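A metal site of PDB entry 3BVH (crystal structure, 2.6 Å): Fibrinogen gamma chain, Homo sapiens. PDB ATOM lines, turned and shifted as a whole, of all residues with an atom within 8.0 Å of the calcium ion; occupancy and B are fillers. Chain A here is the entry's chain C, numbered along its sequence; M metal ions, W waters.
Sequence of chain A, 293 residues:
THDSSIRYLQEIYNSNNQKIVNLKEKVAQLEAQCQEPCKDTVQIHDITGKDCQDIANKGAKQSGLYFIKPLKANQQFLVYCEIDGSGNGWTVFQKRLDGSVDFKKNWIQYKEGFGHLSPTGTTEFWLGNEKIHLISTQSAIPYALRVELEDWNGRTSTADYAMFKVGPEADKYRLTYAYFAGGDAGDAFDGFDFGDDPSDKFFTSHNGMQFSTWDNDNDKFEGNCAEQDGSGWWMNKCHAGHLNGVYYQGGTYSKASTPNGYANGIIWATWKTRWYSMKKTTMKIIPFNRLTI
The side-chain carboxylate of Asp 219 sits at hydrogen-bond distance from the backbone NH of Cys 225 (3.1 Å).
The side-chain sulfur (SG) of Cys 225 is disulfide-bonded to the side-chain sulfur (SG) of Cys 238.
N of Asp 219 lies within hydrogen-bond range of OG of Ser 212.
OD2 of Asp 217 lies close to ND2 of Asn 224.
C of Glu 222 touches the calcium ion, 3.98 Å away.
Five residues have an atom within 4 Å of the calcium ion: Asp 217, Asp 219, Phe 221, Glu 222 and Gly 223.
The calcium ion is bound by O of Phe 221 (2.3 Å), OD1 of Asp 219 (2.3 Å), OD1 of Asp 217 (2.4 Å), O of Gly 223 (2.4 Å), water W1 (2.5 Å) and OD2 of Asp 217 (2.5 Å).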
ATOM      1  N   SER A 212      27.583 -33.703  16.852  1.00  0.00           N
ATOM      2  CA  SER A 212      27.324 -32.414  16.220  1.00  0.00           C
ATOM      3  C   SER A 212      27.827 -32.333  14.779  1.00  0.00           C
ATOM      4  O   SER A 212      28.861 -32.888  14.436  1.00  0.00           O
ATOM      5  CB  SER A 212      27.978 -31.255  17.022  1.00  0.00           C
ATOM      6  OG  SER A 212      27.333 -31.004  18.261  1.00  0.00           O
ATOM      7  N   ASN A 216      23.618 -28.767  12.777  1.00  0.00           N
ATOM      8  CA  ASN A 216      22.976 -29.303  13.975  1.00  0.00           C
ATOM      9  C   ASN A 216      23.991 -29.314  15.118  1.00  0.00           C
ATOM     10  O   ASN A 216      24.620 -30.325  15.420  1.00  0.00           O
ATOM     11  CB  ASN A 216      22.450 -30.704  13.702  1.00  0.00           C
ATOM     12  CG  ASN A 216      21.453 -31.171  14.749  1.00  0.00           C
ATOM     13  OD1 ASN A 216      20.537 -31.923  14.450  1.00  0.00           O
ATOM     14  ND2 ASN A 216      21.659 -30.744  15.978  1.00  0.00           N
ATOM     15  N   ASP A 217      24.122 -28.140  15.752  1.00  0.00           N
ATOM     16  CA  ASP A 217      25.038 -27.864  16.855  1.00  0.00           C
ATOM     17  C   ASP A 217      24.510 -28.377  18.196  1.00  0.00           C
ATOM     18  O   ASP A 217      23.471 -27.939  18.664  1.00  0.00           O
ATOM     19  CB  ASP A 217      25.236 -26.345  16.939  1.00  0.00           C
ATOM     20  CG  ASP A 217      26.313 -25.933  17.922  1.00  0.00           C
ATOM     21  OD1 ASP A 217      26.324 -26.423  19.073  1.00  0.00           O
ATOM     22  OD2 ASP A 217      27.156 -25.092  17.553  1.00  0.00           O
ATOM     23  N   ASN A 218      25.246 -29.304  18.811  1.00  0.00           N
ATOM     24  CA  ASN A 218      24.844 -29.838  20.109  1.00  0.00           C
ATOM     25  C   ASN A 218      26.031 -29.810  21.070  1.00  0.00           C
ATOM     26  O   ASN A 218      26.041 -30.511  22.088  1.00  0.00           O
ATOM     27  CB  ASN A 218      24.336 -31.261  19.961  1.00  0.00           C
ATOM     28  CG  ASN A 218      23.123 -31.354  19.071  1.00  0.00           C
ATOM     29  OD1 ASN A 218      23.133 -32.060  18.067  1.00  0.00           O
ATOM     30  ND2 ASN A 218      22.077 -30.615  19.428  1.00  0.00           N
ATOM     31  N   ASP A 219      27.026 -28.986  20.746  1.00  0.00           N
ATOM     32  CA  ASP A 219      28.234 -28.863  21.559  1.00  0.00           C
ATOM     33  C   ASP A 219      28.053 -27.956  22.789  1.00  0.00           C
ATOM     34  O   ASP A 219      26.984 -27.400  23.014  1.00  0.00           O
ATOM     35  CB  ASP A 219      29.389 -28.352  20.702  1.00  0.00           C
ATOM     36  CG  ASP A 219      29.132 -26.967  20.106  1.00  0.00           C
ATOM     37  OD1 ASP A 219      28.610 -26.088  20.817  1.00  0.00           O
ATOM     38  OD2 ASP A 219      29.460 -26.774  18.917  1.00  0.00           O
ATOM     39  N   LYS A 220      29.123 -27.815  23.565  1.00  0.00           N
ATOM     40  CA  LYS A 220      29.131 -26.999  24.766  1.00  0.00           C
ATOM     41  C   LYS A 220      29.826 -25.667  24.497  1.00  0.00           C
ATOM     42  O   LYS A 220      30.366 -25.038  25.397  1.00  0.00           O
ATOM     43  CB  LYS A 220      29.878 -27.727  25.893  1.00  0.00           C
ATOM     44  CG  LYS A 220      29.268 -29.054  26.275  1.00  0.00           C
ATOM     45  CD  LYS A 220      27.894 -28.858  26.847  1.00  0.00           C
ATOM     46  CE  LYS A 220      27.265 -30.187  27.234  1.00  0.00           C
ATOM     47  NZ  LYS A 220      25.996 -29.984  27.985  1.00  0.00           N
ATOM     48  N   PHE A 221      29.798 -25.243  23.235  1.00  0.00           N
ATOM     49  CA  PHE A 221      30.436 -24.008  22.818  1.00  0.00           C
ATOM     50  C   PHE A 221      29.331 -23.076  22.371  1.00  0.00           C
ATOM     51  O   PHE A 221      28.333 -23.526  21.814  1.00  0.00           O
ATOM     52  CB  PHE A 221      31.395 -24.321  21.668  1.00  0.00           C
ATOM     53  CG  PHE A 221      32.100 -23.126  21.112  1.00  0.00           C
ATOM     54  CD1 PHE A 221      32.506 -22.076  21.930  1.00  0.00           C
ATOM     55  CD2 PHE A 221      32.444 -23.094  19.756  1.00  0.00           C
ATOM     56  CE1 PHE A 221      33.245 -21.004  21.416  1.00  0.00           C
ATOM     57  CE2 PHE A 221      33.189 -22.023  19.230  1.00  0.00           C
ATOM     58  CZ  PHE A 221      33.590 -20.982  20.061  1.00  0.00           C
ATOM     59  N   GLU A 222      29.479 -21.777  22.610  1.00  0.00           N
ATOM     60  CA  GLU A 222      28.449 -20.856  22.165  1.00  0.00           C
ATOM     61  C   GLU A 222      28.590 -20.727  20.650  1.00  0.00           C
ATOM     62  O   GLU A 222      27.644 -20.363  19.976  1.00  0.00           O
ATOM     63  CB  GLU A 222      28.556 -19.485  22.846  1.00  0.00           C
ATOM     64  CG  GLU A 222      29.719 -18.611  22.433  1.00  0.00           C
ATOM     65  CD  GLU A 222      29.648 -17.242  23.114  1.00  0.00           C
ATOM     66  OE1 GLU A 222      30.677 -16.541  23.147  1.00  0.00           O
ATOM     67  OE2 GLU A 222      28.555 -16.859  23.596  1.00  0.00           O
ATOM     68  N   GLY A 223      29.774 -21.041  20.141  1.00  0.00           N
ATOM     69  CA  GLY A 223      29.980 -21.006  18.708  1.00  0.00           C
ATOM     70  C   GLY A 223      29.630 -22.374  18.127  1.00  0.00           C
ATOM     71  O   GLY A 223      28.964 -23.175  18.785  1.00  0.00           O
ATOM     72  N   ASN A 224      30.099 -22.653  16.922  1.00  0.00           N
ATOM     73  CA  ASN A 224      29.807 -23.940  16.279  1.00  0.00           C
ATOM     74  C   ASN A 224      31.089 -24.714  15.966  1.00  0.00           C
ATOM     75  O   ASN A 224      31.711 -24.507  14.922  1.00  0.00           O
ATOM     76  CB  ASN A 224      29.012 -23.696  14.993  1.00  0.00           C
ATOM     77  CG  ASN A 224      28.440 -24.971  14.397  1.00  0.00           C
ATOM     78  OD1 ASN A 224      27.650 -24.916  13.456  1.00  0.00           O
ATOM     79  ND2 ASN A 224      28.834 -26.124  14.926  1.00  0.00           N
ATOM     80  N   CYS A 225      31.483 -25.604  16.883  1.00  0.00           N
ATOM     81  CA  CYS A 225      32.695 -26.410  16.710  1.00  0.00           C
ATOM     82  C   CYS A 225      32.695 -27.159  15.380  1.00  0.00           C
ATOM     83  O   CYS A 225      33.570 -26.975  14.541  1.00  0.00           O
ATOM     84  CB  CYS A 225      32.830 -27.437  17.841  1.00  0.00           C
ATOM     85  SG  CYS A 225      33.048 -26.835  19.543  1.00  0.00           S
ATOM     86  N   ALA A 226      31.702 -28.027  15.206  1.00  0.00           N
ATOM     87  CA  ALA A 226      31.578 -28.836  14.005  1.00  0.00           C
ATOM     88  C   ALA A 226      31.753 -27.987  12.774  1.00  0.00           C
ATOM     89  O   ALA A 226      32.460 -28.363  11.844  1.00  0.00           O
ATOM     90  CB  ALA A 226      30.235 -29.547  13.969  1.00  0.00           C
ATOM     91  N   ASN A 236      32.823 -30.931  22.364  1.00  0.00           N
ATOM     92  CA  ASN A 236      32.619 -30.322  23.670  1.00  0.00           C
ATOM     93  C   ASN A 236      32.790 -28.819  23.417  1.00  0.00           C
ATOM     94  O   ASN A 236      31.834 -28.128  23.083  1.00  0.00           O
ATOM     95  CB  ASN A 236      33.672 -30.804  24.669  1.00  0.00           C
ATOM     96  CG  ASN A 236      33.257 -30.548  26.115  1.00  0.00           C
ATOM     97  OD1 ASN A 236      32.438 -29.670  26.395  1.00  0.00           O
ATOM     98  ND2 ASN A 236      33.815 -31.324  27.051  1.00  0.00           N
ATOM     99  N   CYS A 238      36.526 -27.467  22.326  1.00  0.00           N
ATOM    100  CA  CYS A 238      35.791 -28.262  21.361  1.00  0.00           C
ATOM    101  C   CYS A 238      36.146 -29.753  21.346  1.00  0.00           C
ATOM    102  O   CYS A 238      35.255 -30.592  21.454  1.00  0.00           O
ATOM    103  CB  CYS A 238      35.959 -27.690  19.956  1.00  0.00           C
ATOM    104  SG  CYS A 238      34.980 -26.191  19.601  1.00  0.00           S
HETATM  105 CA    CA M   1      27.236 -24.401  19.934  1.00  0.00          CA
HETATM  106  O   HOH W   1      25.928 -25.451  21.733  1.00  0.00           O
